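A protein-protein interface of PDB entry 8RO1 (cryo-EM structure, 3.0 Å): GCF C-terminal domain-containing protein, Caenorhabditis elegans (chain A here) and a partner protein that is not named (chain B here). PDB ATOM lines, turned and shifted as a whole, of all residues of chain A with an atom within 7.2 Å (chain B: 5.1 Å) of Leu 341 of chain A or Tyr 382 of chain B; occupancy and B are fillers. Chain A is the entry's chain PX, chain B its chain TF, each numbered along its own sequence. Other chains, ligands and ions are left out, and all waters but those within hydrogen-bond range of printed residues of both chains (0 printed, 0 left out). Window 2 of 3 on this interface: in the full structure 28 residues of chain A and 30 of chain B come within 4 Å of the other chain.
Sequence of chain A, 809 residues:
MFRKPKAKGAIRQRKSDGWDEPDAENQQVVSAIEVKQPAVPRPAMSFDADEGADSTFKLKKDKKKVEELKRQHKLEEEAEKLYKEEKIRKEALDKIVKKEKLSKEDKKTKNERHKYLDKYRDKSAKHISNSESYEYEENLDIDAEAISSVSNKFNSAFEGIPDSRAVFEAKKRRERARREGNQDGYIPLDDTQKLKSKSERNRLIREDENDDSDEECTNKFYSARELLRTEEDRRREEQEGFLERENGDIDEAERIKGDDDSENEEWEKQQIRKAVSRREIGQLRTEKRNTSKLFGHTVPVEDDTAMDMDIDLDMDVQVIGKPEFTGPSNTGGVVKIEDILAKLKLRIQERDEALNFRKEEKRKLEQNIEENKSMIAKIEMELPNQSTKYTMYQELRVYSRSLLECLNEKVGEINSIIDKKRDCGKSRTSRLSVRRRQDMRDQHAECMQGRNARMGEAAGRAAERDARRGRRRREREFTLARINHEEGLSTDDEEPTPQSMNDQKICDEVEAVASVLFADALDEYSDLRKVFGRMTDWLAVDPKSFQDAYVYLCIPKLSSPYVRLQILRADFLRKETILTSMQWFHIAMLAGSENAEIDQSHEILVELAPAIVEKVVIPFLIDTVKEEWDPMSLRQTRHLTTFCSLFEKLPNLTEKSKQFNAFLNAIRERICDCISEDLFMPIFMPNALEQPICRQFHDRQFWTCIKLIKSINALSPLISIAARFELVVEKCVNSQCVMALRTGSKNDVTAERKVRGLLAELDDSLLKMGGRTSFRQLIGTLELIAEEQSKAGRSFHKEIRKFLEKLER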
ATOM      1  N   GLU A 338      16.290  -9.230 -31.681  1.00  0.00           N
ATOM      2  CA  GLU A 338      15.052  -8.597 -32.115  1.00  0.00           C
ATOM      3  C   GLU A 338      14.382  -9.438 -33.195  1.00  0.00           C
ATOM      4  O   GLU A 338      13.256  -9.901 -33.037  1.00  0.00           O
ATOM      5  CB  GLU A 338      15.328  -7.189 -32.634  1.00  0.00           C
ATOM      6  CG  GLU A 338      15.995  -6.286 -31.620  1.00  0.00           C
ATOM      7  CD  GLU A 338      16.024  -4.839 -32.068  1.00  0.00           C
ATOM      8  OE1 GLU A 338      15.735  -4.581 -33.254  1.00  0.00           O
ATOM      9  OE2 GLU A 338      16.334  -3.962 -31.236  1.00  0.00           O
ATOM     10  N   ASP A 339      15.103  -9.631 -34.298  1.00  0.00           N
ATOM     11  CA  ASP A 339      14.873 -10.806 -35.137  1.00  0.00           C
ATOM     12  C   ASP A 339      15.272 -12.077 -34.399  1.00  0.00           C
ATOM     13  O   ASP A 339      14.646 -13.129 -34.574  1.00  0.00           O
ATOM     14  CB  ASP A 339      15.631 -10.683 -36.465  1.00  0.00           C
ATOM     15  CG  ASP A 339      17.102 -10.350 -36.285  1.00  0.00           C
ATOM     16  OD1 ASP A 339      17.468  -9.877 -35.188  1.00  0.00           O
ATOM     17  OD2 ASP A 339      17.886 -10.548 -37.237  1.00  0.00           O
ATOM     18  N   ILE A 340      16.317 -11.996 -33.579  1.00  0.00           N
ATOM     19  CA  ILE A 340      16.627 -13.067 -32.634  1.00  0.00           C
ATOM     20  C   ILE A 340      15.444 -13.278 -31.694  1.00  0.00           C
ATOM     21  O   ILE A 340      15.071 -14.416 -31.381  1.00  0.00           O
ATOM     22  CB  ILE A 340      17.935 -12.741 -31.877  1.00  0.00           C
ATOM     23  CG1 ILE A 340      19.113 -12.639 -32.871  1.00  0.00           C
ATOM     24  CG2 ILE A 340      18.243 -13.802 -30.782  1.00  0.00           C
ATOM     25  CD1 ILE A 340      20.426 -12.150 -32.282  1.00  0.00           C
ATOM     26  N   LEU A 341      14.839 -12.183 -31.235  1.00  0.00           N
ATOM     27  CA  LEU A 341      13.669 -12.259 -30.366  1.00  0.00           C
ATOM     28  C   LEU A 341      12.487 -12.909 -31.071  1.00  0.00           C
ATOM     29  O   LEU A 341      11.708 -13.632 -30.440  1.00  0.00           O
ATOM     30  CB  LEU A 341      13.293 -10.850 -29.901  1.00  0.00           C
ATOM     31  CG  LEU A 341      12.413 -10.622 -28.668  1.00  0.00           C
ATOM     32  CD1 LEU A 341      12.699  -9.240 -28.102  1.00  0.00           C
ATOM     33  CD2 LEU A 341      10.922 -10.749 -28.977  1.00  0.00           C
ATOM     34  N   ALA A 342      12.362 -12.702 -32.381  1.00  0.00           N
ATOM     35  CA  ALA A 342      11.344 -13.408 -33.153  1.00  0.00           C
ATOM     36  C   ALA A 342      11.666 -14.893 -33.290  1.00  0.00           C
ATOM     37  O   ALA A 342      10.766 -15.735 -33.175  1.00  0.00           O
ATOM     38  CB  ALA A 342      11.201 -12.763 -34.530  1.00  0.00           C
ATOM     39  N   LYS A 343      12.929 -15.235 -33.550  1.00  0.00           N
ATOM     40  CA  LYS A 343      13.351 -16.632 -33.480  1.00  0.00           C
ATOM     41  C   LYS A 343      13.058 -17.239 -32.113  1.00  0.00           C
ATOM     42  O   LYS A 343      12.703 -18.418 -32.011  1.00  0.00           O
ATOM     43  CB  LYS A 343      14.839 -16.754 -33.795  1.00  0.00           C
ATOM     44  CG  LYS A 343      15.195 -16.510 -35.245  1.00  0.00           C
ATOM     45  CD  LYS A 343      16.689 -16.652 -35.462  1.00  0.00           C
ATOM     46  CE  LYS A 343      17.079 -16.371 -36.900  1.00  0.00           C
ATOM     47  NZ  LYS A 343      18.547 -16.507 -37.099  1.00  0.00           N
ATOM     48  N   LEU A 344      13.203 -16.448 -31.052  1.00  0.00           N
ATOM     49  CA  LEU A 344      12.957 -16.966 -29.710  1.00  0.00           C
ATOM     50  C   LEU A 344      11.477 -17.241 -29.474  1.00  0.00           C
ATOM     51  O   LEU A 344      11.120 -18.253 -28.860  1.00  0.00           O
ATOM     52  CB  LEU A 344      13.464 -15.970 -28.664  1.00  0.00           C
ATOM     53  CG  LEU A 344      14.722 -16.311 -27.866  1.00  0.00           C
ATOM     54  CD1 LEU A 344      15.857 -15.358 -28.214  1.00  0.00           C
ATOM     55  CD2 LEU A 344      14.413 -16.246 -26.388  1.00  0.00           C
ATOM     56  N   LYS A 345      10.604 -16.355 -29.953  1.00  0.00           N
ATOM     57  CA  LYS A 345       9.169 -16.594 -29.848  1.00  0.00           C
ATOM     58  C   LYS A 345       8.753 -17.849 -30.602  1.00  0.00           C
ATOM     59  O   LYS A 345       7.922 -18.626 -30.118  1.00  0.00           O
ATOM     60  CB  LYS A 345       8.395 -15.385 -30.367  1.00  0.00           C
ATOM     61  CG  LYS A 345       8.313 -14.230 -29.391  1.00  0.00           C
ATOM     62  CD  LYS A 345       7.657 -13.023 -30.039  1.00  0.00           C
ATOM     63  CE  LYS A 345       7.409 -11.909 -29.040  1.00  0.00           C
ATOM     64  NZ  LYS A 345       6.791 -10.716 -29.681  1.00  0.00           N
ATOM     65  N   LEU A 346       9.331 -18.067 -31.784  1.00  0.00           N
ATOM     66  CA  LEU A 346       9.126 -19.324 -32.496  1.00  0.00           C
ATOM     67  C   LEU A 346       9.583 -20.519 -31.671  1.00  0.00           C
ATOM     68  O   LEU A 346       8.885 -21.537 -31.606  1.00  0.00           O
ATOM     69  CB  LEU A 346       9.867 -19.279 -33.835  1.00  0.00           C
ATOM     70  CG  LEU A 346       9.905 -20.554 -34.688  1.00  0.00           C
ATOM     71  CD1 LEU A 346       9.789 -20.199 -36.162  1.00  0.00           C
ATOM     72  CD2 LEU A 346      11.192 -21.359 -34.467  1.00  0.00           C
ATOM     73  N   ARG A 347      10.745 -20.415 -31.029  1.00  0.00           N
ATOM     74  CA  ARG A 347      11.211 -21.512 -30.190  1.00  0.00           C
ATOM     75  C   ARG A 347      10.297 -21.720 -28.993  1.00  0.00           C
ATOM     76  O   ARG A 347      10.100 -22.858 -28.554  1.00  0.00           O
ATOM     77  CB  ARG A 347      12.643 -21.242 -29.731  1.00  0.00           C
ATOM     78  CG  ARG A 347      13.691 -21.535 -30.794  1.00  0.00           C
ATOM     79  CD  ARG A 347      13.919 -23.027 -30.991  1.00  0.00           C
ATOM     80  NE  ARG A 347      14.927 -23.282 -32.021  1.00  0.00           N
ATOM     81  CZ  ARG A 347      16.063 -23.960 -31.878  1.00  0.00           C
ATOM     82  NH1 ARG A 347      16.863 -24.103 -32.930  1.00  0.00           N
ATOM     83  NH2 ARG A 347      16.429 -24.501 -30.723  1.00  0.00           N
ATOM     84  N   ILE A 348       9.735 -20.637 -28.459  1.00  0.00           N
ATOM     85  CA  ILE A 348       8.791 -20.746 -27.352  1.00  0.00           C
ATOM     86  C   ILE A 348       7.532 -21.485 -27.793  1.00  0.00           C
ATOM     87  O   ILE A 348       7.020 -22.353 -27.076  1.00  0.00           O
ATOM     88  CB  ILE A 348       8.480 -19.336 -26.802  1.00  0.00           C
ATOM     89  CG1 ILE A 348       9.655 -18.844 -25.951  1.00  0.00           C
ATOM     90  CG2 ILE A 348       7.160 -19.299 -25.992  1.00  0.00           C
ATOM     91  CD1 ILE A 348       9.667 -17.345 -25.702  1.00  0.00           C
ATOM     92  N   ILE B 378      14.827 -20.353 -21.312  1.00  0.00           N
ATOM     93  CA  ILE B 378      14.297 -19.628 -22.463  1.00  0.00           C
ATOM     94  C   ILE B 378      13.482 -18.426 -22.007  1.00  0.00           C
ATOM     95  O   ILE B 378      13.567 -17.342 -22.595  1.00  0.00           O
ATOM     96  CB  ILE B 378      13.472 -20.587 -23.346  1.00  0.00           C
ATOM     97  CG1 ILE B 378      14.401 -21.595 -24.036  1.00  0.00           C
ATOM     98  CG2 ILE B 378      12.649 -19.816 -24.398  1.00  0.00           C
ATOM     99  CD1 ILE B 378      13.703 -22.841 -24.554  1.00  0.00           C
ATOM    100  N   LYS B 379      12.681 -18.592 -20.954  1.00  0.00           N
ATOM    101  CA  LYS B 379      11.897 -17.471 -20.448  1.00  0.00           C
ATOM    102  C   LYS B 379      12.779 -16.367 -19.887  1.00  0.00           C
ATOM    103  O   LYS B 379      12.434 -15.186 -20.004  1.00  0.00           O
ATOM    104  CB  LYS B 379      10.933 -17.934 -19.350  1.00  0.00           C
ATOM    105  CG  LYS B 379       9.714 -18.704 -19.839  1.00  0.00           C
ATOM    106  CD  LYS B 379       8.712 -19.079 -18.732  1.00  0.00           C
ATOM    107  CE  LYS B 379       9.290 -20.009 -17.670  1.00  0.00           C
ATOM    108  NZ  LYS B 379       8.268 -20.365 -16.645  1.00  0.00           N
ATOM    109  N   ASP B 380      13.912 -16.719 -19.280  1.00  0.00           N
ATOM    110  CA  ASP B 380      14.777 -15.704 -18.689  1.00  0.00           C
ATOM    111  C   ASP B 380      15.395 -14.784 -19.737  1.00  0.00           C
ATOM    112  O   ASP B 380      15.333 -13.557 -19.604  1.00  0.00           O
ATOM    113  CB  ASP B 380      15.876 -16.387 -17.880  1.00  0.00           C
ATOM    114  CG  ASP B 380      15.354 -17.036 -16.613  1.00  0.00           C
ATOM    115  OD1 ASP B 380      14.182 -16.802 -16.247  1.00  0.00           O
ATOM    116  OD2 ASP B 380      16.120 -17.797 -15.987  1.00  0.00           O
ATOM    117  N   VAL B 381      15.982 -15.345 -20.796  1.00  0.00           N
ATOM    118  CA  VAL B 381      16.583 -14.486 -21.816  1.00  0.00           C
ATOM    119  C   VAL B 381      15.515 -13.685 -22.548  1.00  0.00           C
ATOM    120  O   VAL B 381      15.715 -12.505 -22.858  1.00  0.00           O
ATOM    121  CB  VAL B 381      17.470 -15.300 -22.782  1.00  0.00           C
ATOM    122  CG1 VAL B 381      18.688 -15.795 -22.055  1.00  0.00           C
ATOM    123  CG2 VAL B 381      16.743 -16.477 -23.416  1.00  0.00           C
ATOM    124  N   TYR B 382      14.366 -14.300 -22.824  1.00  0.00           N
ATOM    125  CA  TYR B 382      13.298 -13.599 -23.526  1.00  0.00           C
ATOM    126  C   TYR B 382      12.759 -12.437 -22.703  1.00  0.00           C
ATOM    127  O   TYR B 382      12.632 -11.313 -23.201  1.00  0.00           O
ATOM    128  CB  TYR B 382      12.187 -14.605 -23.845  1.00  0.00           C
ATOM    129  CG  TYR B 382      10.909 -14.029 -24.416  1.00  0.00           C
ATOM    130  CD1 TYR B 382      10.842 -13.558 -25.718  1.00  0.00           C
ATOM    131  CD2 TYR B 382       9.752 -13.994 -23.646  1.00  0.00           C
ATOM    132  CE1 TYR B 382       9.659 -13.048 -26.231  1.00  0.00           C
ATOM    133  CE2 TYR B 382       8.573 -13.489 -24.145  1.00  0.00           C
ATOM    134  CZ  TYR B 382       8.528 -13.019 -25.436  1.00  0.00           C
ATOM    135  OH  TYR B 382       7.345 -12.516 -25.922  1.00  0.00           O
ATOM    136  N   GLU B 383      12.446 -12.689 -21.431  1.00  0.00           N
ATOM    137  CA  GLU B 383      11.872 -11.644 -20.588  1.00  0.00           C
ATOM    138  C   GLU B 383      12.865 -10.527 -20.288  1.00  0.00           C
ATOM    139  O   GLU B 383      12.483  -9.352 -20.240  1.00  0.00           O
ATOM    140  CB  GLU B 383      11.330 -12.249 -19.295  1.00  0.00           C
ATOM    141  CG  GLU B 383      10.021 -13.001 -19.486  1.00  0.00           C
ATOM    142  CD  GLU B 383       9.546 -13.686 -18.222  1.00  0.00           C
ATOM    143  OE1 GLU B 383      10.053 -13.343 -17.134  1.00  0.00           O
ATOM    144  OE2 GLU B 383       8.653 -14.554 -18.317  1.00  0.00           O
ATOM    145  N   LEU B 384      14.140 -10.863 -20.076  1.00  0.00           N
ATOM    146  CA  LEU B 384      15.110  -9.824 -19.741  1.00  0.00           C
ATOM    147  C   LEU B 384      15.415  -8.925 -20.932  1.00  0.00           C
ATOM    148  O   LEU B 384      15.502  -7.702 -20.783  1.00  0.00           O
ATOM    149  CB  LEU B 384      16.394 -10.455 -19.203  1.00  0.00           C
ATOM    150  CG  LEU B 384      16.478 -10.620 -17.679  1.00  0.00           C
ATOM    151  CD1 LEU B 384      15.328 -11.446 -17.087  1.00  0.00           C
ATOM    152  CD2 LEU B 384      17.822 -11.237 -17.308  1.00  0.00           C
ATOM    153  N   ILE B 385      15.580  -9.505 -22.119  1.00  0.00           N
ATOM    154  CA  ILE B 385      15.844  -8.696 -23.303  1.00  0.00           C
ATOM    155  C   ILE B 385      14.601  -7.894 -23.670  1.00  0.00           C
ATOM    156  O   ILE B 385      14.696  -6.749 -24.128  1.00  0.00           O
ATOM    157  CB  ILE B 385      16.353  -9.582 -24.462  1.00  0.00           C
ATOM    158  CG1 ILE B 385      17.702 -10.224 -24.087  1.00  0.00           C
ATOM    159  CG2 ILE B 385      16.513  -8.771 -25.772  1.00  0.00           C
ATOM    160  CD1 ILE B 385      18.158 -11.347 -25.006  1.00  0.00           C
ATOM    161  N   ASP B 386      13.420  -8.487 -23.480  1.00  0.00           N
ATOM    162  CA  ASP B 386      12.166  -7.782 -23.727  1.00  0.00           C
ATOM    163  C   ASP B 386      12.020  -6.580 -22.801  1.00  0.00           C
ATOM    164  O   ASP B 386      11.665  -5.482 -23.244  1.00  0.00           O
ATOM    165  CB  ASP B 386      10.988  -8.740 -23.549  1.00  0.00           C
ATOM    166  CG  ASP B 386       9.650  -8.066 -23.774  1.00  0.00           C
ATOM    167  OD1 ASP B 386       9.577  -7.162 -24.632  1.00  0.00           O
ATOM    168  OD2 ASP B 386       8.671  -8.441 -23.094  1.00  0.00           O
ATOM    169  N   GLY B 387      12.269  -6.777 -21.505  1.00  0.00           N
ATOM    170  CA  GLY B 387      12.302  -5.643 -20.593  1.00  0.00           C
ATOM    171  C   GLY B 387      13.364  -4.635 -20.986  1.00  0.00           C
ATOM    172  O   GLY B 387      13.167  -3.426 -20.852  1.00  0.00           O
ATOM    173  N   SER B 389      14.294  -4.210 -24.113  1.00  0.00           N
ATOM    174  CA  SER B 389      13.820  -3.603 -25.350  1.00  0.00           C
ATOM    175  C   SER B 389      12.805  -2.504 -25.061  1.00  0.00           C
ATOM    176  O   SER B 389      12.628  -1.598 -25.883  1.00  0.00           O
ATOM    177  CB  SER B 389      13.216  -4.660 -26.270  1.00  0.00           C
ATOM    178  OG  SER B 389      11.906  -5.004 -25.859  1.00  0.00           O
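Leu 341 of chain A touches Tyr 382 of chain B. Val 381 of chain B touches Leu 344 of chain A. Tyr 382 of chain B touches Leu 344 of chain A. Lys 345 of chain A touches Tyr 382 of chain B. CG2 of Ile 378 of chain B touches CG1 of Ile 348 of chain A, at 3.5 Å. CG of Tyr 382 of chain B touches CD1 of Ile 348 of chain A (3.8 Å).
Leu 341 of chain A touches just one residue of chain B: Tyr 382. Tyr 382 of chain B touches just these residues of chain A: Leu 341 (3.8 Å), Leu 344 (3.8 Å), Lys 345 (3.2 Å) and Ile 348 (3.8 Å). Printed residues of chain A within 4 Å of Ile 378 of chain B: Ile 348 (3.5 Å). Printed residues of chain B within 4 Å of Leu 344 of chain A: Val 381 and Tyr 382. Of the printed residues of chain B, Lys 345 of chain A touches Tyr 382 (3.2 Å). Of the printed residues of chain A, Val 381 of chain B touches Leu 344 (3.8 Å). Gly 387 of chain B touches none of the printed residues of chain A. The nearest residue of chain B that does not touch Leu 341 of chain A is Ile 385 of chain B (4.5 Å).
Of the 11 printed residues of chain B, 3 touch a printed residue of chain A. Hydrophobic or aromatic side chains of chain B that line the printed part of chain A: Ile 378, Val 381 and Tyr 382. Along chain B the printed residues that touch a printed residue of chain A span positions 378 to 382. Of the 11 printed residues of chain A, 4 touch a printed residue of chain B. Hydrophobic or aromatic side chains of chain A that line the printed part of chain B: Leu 341, Leu 344 and Ile 348.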
